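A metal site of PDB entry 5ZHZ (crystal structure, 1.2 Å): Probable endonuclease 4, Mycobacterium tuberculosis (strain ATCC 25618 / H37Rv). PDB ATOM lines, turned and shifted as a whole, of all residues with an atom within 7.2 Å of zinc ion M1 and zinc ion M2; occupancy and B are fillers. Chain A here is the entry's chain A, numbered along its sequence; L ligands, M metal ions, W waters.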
ATOM      1  N   GLN A  25      15.234  12.444  24.408  1.00  0.00           N
ATOM      2  CA  GLN A  25      14.783  11.212  23.786  1.00  0.00           C
ATOM      3  C   GLN A  25      15.801  10.846  22.702  1.00  0.00           C
ATOM      4  O   GLN A  25      16.309  11.736  22.003  1.00  0.00           O
ATOM      5  CB  GLN A  25      13.408  11.414  23.185  1.00  0.00           C
ATOM      6  CG  GLN A  25      12.766  10.163  22.587  1.00  0.00           C
ATOM      7  CD  GLN A  25      11.421  10.502  22.028  1.00  0.00           C
ATOM      8  OE1 GLN A  25      10.388  10.408  22.732  1.00  0.00           O
ATOM      9  NE2 GLN A  25      11.383  10.959  20.767  1.00  0.00           N
ATOM     10  N   PHE A  27      17.070   7.491  19.787  1.00  0.00           N
ATOM     11  CA  PHE A  27      17.069   6.134  19.247  1.00  0.00           C
ATOM     12  C   PHE A  27      18.316   5.413  19.699  1.00  0.00           C
ATOM     13  O   PHE A  27      19.388   5.990  19.880  1.00  0.00           O
ATOM     14  CB  PHE A  27      17.051   6.146  17.715  1.00  0.00           C
ATOM     15  CG  PHE A  27      15.724   6.594  17.124  1.00  0.00           C
ATOM     16  CD1 PHE A  27      14.739   5.642  16.891  1.00  0.00           C
ATOM     17  CD2 PHE A  27      15.459   7.912  16.857  1.00  0.00           C
ATOM     18  CE1 PHE A  27      13.521   5.992  16.347  1.00  0.00           C
ATOM     19  CE2 PHE A  27      14.193   8.250  16.303  1.00  0.00           C
ATOM     20  CZ  PHE A  27      13.255   7.296  16.090  1.00  0.00           C
ATOM     21  N   HIS A  56      13.052   6.057  21.733  1.00  0.00           N
ATOM     22  CA  HIS A  56      12.121   5.823  20.647  1.00  0.00           C
ATOM     23  C   HIS A  56      12.425   4.491  19.983  1.00  0.00           C
ATOM     24  O   HIS A  56      13.573   4.260  19.581  1.00  0.00           O
ATOM     25  CB  HIS A  56      12.214   6.975  19.626  1.00  0.00           C
ATOM     26  CG  HIS A  56      11.008   7.108  18.748  1.00  0.00           C
ATOM     27  ND1 HIS A  56      10.505   6.067  17.973  1.00  0.00           N
ATOM     28  CD2 HIS A  56      10.177   8.159  18.534  1.00  0.00           C
ATOM     29  CE1 HIS A  56       9.420   6.495  17.345  1.00  0.00           C
ATOM     30  NE2 HIS A  56       9.199   7.766  17.646  1.00  0.00           N
ATOM     31  N   ALA A  57      11.442   3.600  19.897  1.00  0.00           N
ATOM     32  CA  ALA A  57      11.653   2.331  19.238  1.00  0.00           C
ATOM     33  C   ALA A  57      11.766   2.546  17.720  1.00  0.00           C
ATOM     34  O   ALA A  57      11.214   3.511  17.189  1.00  0.00           O
ATOM     35  CB  ALA A  57      10.476   1.404  19.531  1.00  0.00           C
ATOM     36  N   TYR A  59      11.349   2.884  13.792  1.00  0.00           N
ATOM     37  CA  TYR A  59      10.152   3.305  13.071  1.00  0.00           C
ATOM     38  C   TYR A  59       9.463   2.175  12.327  1.00  0.00           C
ATOM     39  O   TYR A  59       8.253   2.262  12.079  1.00  0.00           O
ATOM     40  CB  TYR A  59      10.549   4.294  12.010  1.00  0.00           C
ATOM     41  CG  TYR A  59      10.832   5.670  12.534  1.00  0.00           C
ATOM     42  CD1 TYR A  59       9.929   6.322  13.419  1.00  0.00           C
ATOM     43  CD2 TYR A  59      11.980   6.362  12.164  1.00  0.00           C
ATOM     44  CE1 TYR A  59      10.169   7.618  13.870  1.00  0.00           C
ATOM     45  CE2 TYR A  59      12.214   7.656  12.644  1.00  0.00           C
ATOM     46  CZ  TYR A  59      11.307   8.274  13.456  1.00  0.00           C
ATOM     47  OH  TYR A  59      11.581   9.545  13.892  1.00  0.00           O
ATOM     48  N   ILE A  94       8.963   4.574  23.440  1.00  0.00           N
ATOM     49  CA  ILE A  94       7.864   5.077  22.629  1.00  0.00           C
ATOM     50  C   ILE A  94       7.803   4.276  21.338  1.00  0.00           C
ATOM     51  O   ILE A  94       8.818   4.090  20.668  1.00  0.00           O
ATOM     52  CB  ILE A  94       8.090   6.577  22.322  1.00  0.00           C
ATOM     53  CG1 ILE A  94       8.027   7.446  23.583  1.00  0.00           C
ATOM     54  CG2 ILE A  94       7.002   7.085  21.372  1.00  0.00           C
ATOM     55  CD1 ILE A  94       9.244   7.415  24.437  1.00  0.00           C
ATOM     56  N   VAL A  95       6.606   3.827  20.965  1.00  0.00           N
ATOM     57  CA  VAL A  95       6.438   3.064  19.727  1.00  0.00           C
ATOM     58  C   VAL A  95       5.221   3.597  18.987  1.00  0.00           C
ATOM     59  O   VAL A  95       4.187   3.904  19.587  1.00  0.00           O
ATOM     60  CB  VAL A  95       6.337   1.555  20.027  1.00  0.00           C
ATOM     61  CG1 VAL A  95       5.181   1.248  20.861  1.00  0.00           C
ATOM     62  CG2 VAL A  95       6.267   0.745  18.753  1.00  0.00           C
ATOM     63  N   HIS A  96       5.329   3.721  17.678  1.00  0.00           N
ATOM     64  CA  HIS A  96       4.226   4.188  16.865  1.00  0.00           C
ATOM     65  C   HIS A  96       3.097   3.162  16.806  1.00  0.00           C
ATOM     66  O   HIS A  96       3.297   1.947  16.953  1.00  0.00           O
ATOM     67  CB  HIS A  96       4.744   4.565  15.493  1.00  0.00           C
ATOM     68  CG  HIS A  96       5.615   5.888  15.517  1.00  0.00           C
ATOM     69  ND1 HIS A  96       5.860   6.406  14.293  1.00  0.00           N
ATOM     70  CD2 HIS A  96       6.245   6.858  16.446  1.00  0.00           C
ATOM     71  CE1 HIS A  96       6.598   7.492  14.473  1.00  0.00           C
ATOM     72  NE2 HIS A  96       6.776   7.744  15.742  1.00  0.00           N
ATOM     73  N   GLU A 129       2.467   6.082  20.384  1.00  0.00           N
ATOM     74  CA  GLU A 129       2.412   7.421  19.812  1.00  0.00           C
ATOM     75  C   GLU A 129       1.486   7.447  18.585  1.00  0.00           C
ATOM     76  O   GLU A 129       1.529   6.551  17.728  1.00  0.00           O
ATOM     77  CB  GLU A 129       3.847   7.849  19.383  1.00  0.00           C
ATOM     78  CG  GLU A 129       3.914   9.297  18.880  1.00  0.00           C
ATOM     79  CD  GLU A 129       5.256   9.708  18.270  1.00  0.00           C
ATOM     80  OE1 GLU A 129       6.208   8.891  18.385  1.00  0.00           O
ATOM     81  OE2 GLU A 129       5.335  10.811  17.672  1.00  0.00           O
ATOM     82  N   ASN A 130       0.680   8.504  18.499  1.00  0.00           N
ATOM     83  CA  ASN A 130      -0.140   8.724  17.311  1.00  0.00           C
ATOM     84  C   ASN A 130       0.724   9.071  16.107  1.00  0.00           C
ATOM     85  O   ASN A 130       1.843   9.590  16.253  1.00  0.00           O
ATOM     86  CB  ASN A 130      -1.202   9.785  17.532  1.00  0.00           C
ATOM     87  CG  ASN A 130      -0.628  11.143  17.877  1.00  0.00           C
ATOM     88  OD1 ASN A 130       0.153  11.282  18.808  1.00  0.00           O
ATOM     89  ND2 ASN A 130      -1.077  12.165  17.164  1.00  0.00           N
ATOM     90  N   THR A 131       0.170   8.840  14.899  1.00  0.00           N
ATOM     91  CA  THR A 131       0.931   8.965  13.655  1.00  0.00           C
ATOM     92  C   THR A 131       0.262   9.931  12.693  1.00  0.00           C
ATOM     93  O   THR A 131      -0.882  10.325  12.858  1.00  0.00           O
ATOM     94  CB  THR A 131       1.111   7.571  13.025  1.00  0.00           C
ATOM     95  OG1 THR A 131      -0.180   6.967  12.831  1.00  0.00           O
ATOM     96  CG2 THR A 131       1.954   6.673  13.921  1.00  0.00           C
ATOM     97  N   CYS A 160       1.665   8.721  24.039  1.00  0.00           N
ATOM     98  CA  CYS A 160       2.454   9.883  23.702  1.00  0.00           C
ATOM     99  C   CYS A 160       1.743  10.650  22.601  1.00  0.00           C
ATOM    100  O   CYS A 160       1.498  10.103  21.510  1.00  0.00           O
ATOM    101  CB  CYS A 160       3.838   9.428  23.193  1.00  0.00           C
ATOM    102  SG  CYS A 160       4.837  10.781  22.549  1.00  0.00           S
ATOM    103  N   LEU A 161       1.398  11.911  22.877  1.00  0.00           N
ATOM    104  CA  LEU A 161       0.721  12.756  21.899  1.00  0.00           C
ATOM    105  C   LEU A 161       1.746  13.589  21.134  1.00  0.00           C
ATOM    106  O   LEU A 161       2.491  14.373  21.741  1.00  0.00           O
ATOM    107  CB  LEU A 161      -0.281  13.681  22.614  1.00  0.00           C
ATOM    108  CG  LEU A 161      -1.029  14.597  21.635  1.00  0.00           C
ATOM    109  CD1 LEU A 161      -1.969  13.804  20.695  1.00  0.00           C
ATOM    110  CD2 LEU A 161      -1.881  15.628  22.384  1.00  0.00           C
ATOM    111  N   ASP A 162       1.790  13.430  19.800  1.00  0.00           N
ATOM    112  CA  ASP A 162       2.672  14.224  18.966  1.00  0.00           C
ATOM    113  C   ASP A 162       1.820  15.286  18.269  1.00  0.00           C
ATOM    114  O   ASP A 162       0.847  14.961  17.547  1.00  0.00           O
ATOM    115  CB  ASP A 162       3.394  13.323  17.973  1.00  0.00           C
ATOM    116  CG  ASP A 162       4.458  14.083  17.152  1.00  0.00           C
ATOM    117  OD1 ASP A 162       4.067  15.094  16.521  1.00  0.00           O
ATOM    118  OD2 ASP A 162       5.621  13.651  17.162  1.00  0.00           O
ATOM    119  N   THR A 163       2.153  16.561  18.513  1.00  0.00           N
ATOM    120  CA  THR A 163       1.332  17.643  17.976  1.00  0.00           C
ATOM    121  C   THR A 163       1.437  17.773  16.462  1.00  0.00           C
ATOM    122  O   THR A 163       0.461  18.204  15.825  1.00  0.00           O
ATOM    123  CB  THR A 163       1.688  18.987  18.624  1.00  0.00           C
ATOM    124  OG1 THR A 163       3.091  19.250  18.437  1.00  0.00           O
ATOM    125  CG2 THR A 163       1.430  18.943  20.143  1.00  0.00           C
ATOM    126  N   CYS A 164       2.602  17.498  15.879  1.00  0.00           N
ATOM    127  CA  CYS A 164       2.695  17.547  14.421  1.00  0.00           C
ATOM    128  C   CYS A 164       1.825  16.460  13.807  1.00  0.00           C
ATOM    129  O   CYS A 164       1.129  16.686  12.797  1.00  0.00           O
ATOM    130  CB  CYS A 164       4.161  17.417  13.973  1.00  0.00           C
ATOM    131  SG  CYS A 164       4.397  17.489  12.146  1.00  0.00           S
ATOM    132  N   HIS A 165       1.858  15.268  14.392  1.00  0.00           N
ATOM    133  CA  HIS A 165       1.059  14.171  13.863  1.00  0.00           C
ATOM    134  C   HIS A 165      -0.425  14.494  13.949  1.00  0.00           C
ATOM    135  O   HIS A 165      -1.193  14.228  13.005  1.00  0.00           O
ATOM    136  CB  HIS A 165       1.410  12.843  14.543  1.00  0.00           C
ATOM    137  CG  HIS A 165       2.857  12.491  14.367  1.00  0.00           C
ATOM    138  ND1 HIS A 165       3.469  11.403  14.935  1.00  0.00           N
ATOM    139  CD2 HIS A 165       3.832  13.134  13.645  1.00  0.00           C
ATOM    140  CE1 HIS A 165       4.766  11.410  14.624  1.00  0.00           C
ATOM    141  NE2 HIS A 165       5.012  12.456  13.831  1.00  0.00           N
ATOM    142  N   VAL A 190       4.470  14.332  25.758  1.00  0.00           N
ATOM    143  CA  VAL A 190       4.070  15.109  24.574  1.00  0.00           C
ATOM    144  C   VAL A 190       5.281  15.316  23.695  1.00  0.00           C
ATOM    145  O   VAL A 190       6.361  15.686  24.215  1.00  0.00           O
ATOM    146  CB  VAL A 190       3.432  16.453  24.981  1.00  0.00           C
ATOM    147  CG1 VAL A 190       3.286  17.388  23.803  1.00  0.00           C
ATOM    148  CG2 VAL A 190       2.090  16.205  25.630  1.00  0.00           C
ATOM    149  N   HIS A 191       5.121  15.081  22.400  1.00  0.00           N
ATOM    150  CA  HIS A 191       6.109  15.505  21.416  1.00  0.00           C
ATOM    151  C   HIS A 191       5.595  16.822  20.867  1.00  0.00           C
ATOM    152  O   HIS A 191       4.567  16.853  20.162  1.00  0.00           O
ATOM    153  CB  HIS A 191       6.236  14.474  20.304  1.00  0.00           C
ATOM    154  CG  HIS A 191       6.915  13.219  20.714  1.00  0.00           C
ATOM    155  ND1 HIS A 191       7.002  12.113  19.876  1.00  0.00           N
ATOM    156  CD2 HIS A 191       7.548  12.897  21.871  1.00  0.00           C
ATOM    157  CE1 HIS A 191       7.697  11.180  20.507  1.00  0.00           C
ATOM    158  NE2 HIS A 191       8.044  11.619  21.715  1.00  0.00           N
ATOM    159  N   CYS A 192       6.261  17.918  21.228  1.00  0.00           N
ATOM    160  CA  CYS A 192       5.807  19.243  20.854  1.00  0.00           C
ATOM    161  C   CYS A 192       6.592  19.711  19.630  1.00  0.00           C
ATOM    162  O   CYS A 192       7.708  20.252  19.746  1.00  0.00           O
ATOM    163  CB  CYS A 192       5.943  20.233  22.005  1.00  0.00           C
ATOM    164  SG  CYS A 192       5.207  21.845  21.610  1.00  0.00           S
ATOM    165  N   ASN A 193       5.983  19.502  18.474  1.00  0.00           N
ATOM    166  CA  ASN A 193       6.552  19.775  17.148  1.00  0.00           C
ATOM    167  C   ASN A 193       5.639  20.707  16.372  1.00  0.00           C
ATOM    168  O   ASN A 193       4.430  20.510  16.356  1.00  0.00           O
ATOM    169  CB  ASN A 193       6.651  18.448  16.383  1.00  0.00           C
ATOM    170  CG  ASN A 193       7.520  17.451  17.076  1.00  0.00           C
ATOM    171  OD1 ASN A 193       8.575  17.811  17.621  1.00  0.00           O
ATOM    172  ND2 ASN A 193       7.086  16.182  17.089  1.00  0.00           N
ATOM    173  N   ASP A 204       4.654  14.277   7.321  1.00  0.00           N
ATOM    174  CA  ASP A 204       5.267  14.369   8.656  1.00  0.00           C
ATOM    175  C   ASP A 204       6.595  15.084   8.536  1.00  0.00           C
ATOM    176  O   ASP A 204       7.660  14.433   8.405  1.00  0.00           O
ATOM    177  CB  ASP A 204       5.457  13.070   9.256  1.00  0.00           C
ATOM    178  CG  ASP A 204       5.960  13.254  10.706  1.00  0.00           C
ATOM    179  OD1 ASP A 204       5.501  14.174  11.383  1.00  0.00           O
ATOM    180  OD2 ASP A 204       6.752  12.490  11.211  1.00  0.00           O
ATOM    181  N   HIS A 206       8.533  17.843  10.592  1.00  0.00           N
ATOM    182  CA  HIS A 206       8.536  18.684  11.792  1.00  0.00           C
ATOM    183  C   HIS A 206       9.188  20.017  11.488  1.00  0.00           C
ATOM    184  O   HIS A 206      10.025  20.140  10.595  1.00  0.00           O
ATOM    185  CB  HIS A 206       9.298  17.999  12.927  1.00  0.00           C
ATOM    186  CG  HIS A 206       8.754  16.638  13.322  1.00  0.00           C
ATOM    187  ND1 HIS A 206       9.280  15.940  14.380  1.00  0.00           N
ATOM    188  CD2 HIS A 206       7.774  15.830  12.812  1.00  0.00           C
ATOM    189  CE1 HIS A 206       8.646  14.784  14.512  1.00  0.00           C
ATOM    190  NE2 HIS A 206       7.714  14.667  13.563  1.00  0.00           N
ATOM    191  N   ILE A 231       9.024  16.535  24.755  1.00  0.00           N
ATOM    192  CA  ILE A 231      10.150  16.373  23.842  1.00  0.00           C
ATOM    193  C   ILE A 231       9.878  17.213  22.605  1.00  0.00           C
ATOM    194  O   ILE A 231       8.888  16.977  21.894  1.00  0.00           O
ATOM    195  CB  ILE A 231      10.326  14.917  23.403  1.00  0.00           C
ATOM    196  CG1 ILE A 231      10.304  13.897  24.525  1.00  0.00           C
ATOM    197  CG2 ILE A 231      11.548  14.777  22.510  1.00  0.00           C
ATOM    198  CD1 ILE A 231      11.287  14.096  25.507  1.00  0.00           C
ATOM    199  N   GLU A 233      10.953  17.476  18.960  1.00  0.00           N
ATOM    200  CA  GLU A 233      11.618  16.634  17.969  1.00  0.00           C
ATOM    201  C   GLU A 233      11.870  17.465  16.720  1.00  0.00           C
ATOM    202  O   GLU A 233      11.466  17.160  15.599  1.00  0.00           O
ATOM    203  CB  GLU A 233      10.766  15.399  17.628  1.00  0.00           C
ATOM    204  CG  GLU A 233      10.367  14.590  18.840  1.00  0.00           C
ATOM    205  CD  GLU A 233       9.508  13.434  18.460  1.00  0.00           C
ATOM    206  OE1 GLU A 233       8.422  13.641  17.893  1.00  0.00           O
ATOM    207  OE2 GLU A 233       9.932  12.289  18.652  1.00  0.00           O
HETATM  208  S1  LIG L   1       8.408  11.214  14.876  1.00  0.00           S
HETATM  209  O1  LIG L   1       9.848  11.441  15.102  1.00  0.00           O
HETATM  210  O2  LIG L   1       7.542  12.179  15.620  1.00  0.00           O
HETATM  211  O3  LIG L   1       8.000   9.828  15.102  1.00  0.00           O
HETATM  212  O4  LIG L   1       8.082  11.521  13.452  1.00  0.00           O
HETATM  213 ZN    ZN M   1       6.922  12.137  17.690  1.00  0.00          ZN
HETATM  214 ZN    ZN M   2       7.647   8.962  16.993  1.00  0.00          ZN
HETATM  215 ZN    ZN M   3       6.788  12.973  13.136  1.00  0.00          ZN
HETATM  216  O   HOH W   1       8.356  10.611  17.805  1.00  0.00           O
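Merely in contact with zinc ion M1: His 165.
Zinc ion M2 is bound by NE2 of His 96. Zinc ion M2 is bound by water W1. Zinc ion M2 is bound by the side-chain carboxylate (OE1) of Glu 129, 2.0 Å away. NE2 of His 56 binds zinc ion M2, at 2.1 Å. Zinc ion M2 is bound by an oxygen (O3) of the ligand.
Zinc ion M1 is bound by OD2 of Asp 162 (2.1 Å), OE2 of Glu 129 (2.1 Å), water W1 (2.1 Å), OE1 of Glu 233 (2.1 Å), O2 of the ligand (2.2 Å) and ND1 of His 191 (2.2 Å). Zinc ion M1 has six donor atoms within binding distance.
OE2 of Glu 129 lies close to ND1 of His 165, at 3.4 Å. The side-chain amide oxygen of Asn 130 sits at hydrogen-bond distance from the backbone NH of Asp 162 (2.9 Å). OD1 of Asp 162 sits at hydrogen-bond distance from N of Cys 164 (2.9 Å). The backbone NH (N) of Glu 233 lies within hydrogen-bond range of the side-chain amide oxygen (OD1) of Asn 193 (2.7 Å). The side-chain sulfur (SG) of Cys 160 lies within hydrogen-bond range of a ring nitrogen (NE2) of His 191 (3.4 Å). OE1 of Gln 25 lies within hydrogen-bond range of NE2 of His 191, 2.8 Å away. The backbone NH of Thr 163 lies within hydrogen-bond range of the backbone carbonyl oxygen of His 191 (2.9 Å). The backbone carbonyl oxygen (O) of Asn 130 is in hydrogen-bond range of a ring nitrogen (ND1) of His 165 (2.8 Å).
The nearest printed residue that does not touch zinc ion M2 is His 191 (4.2 Å).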
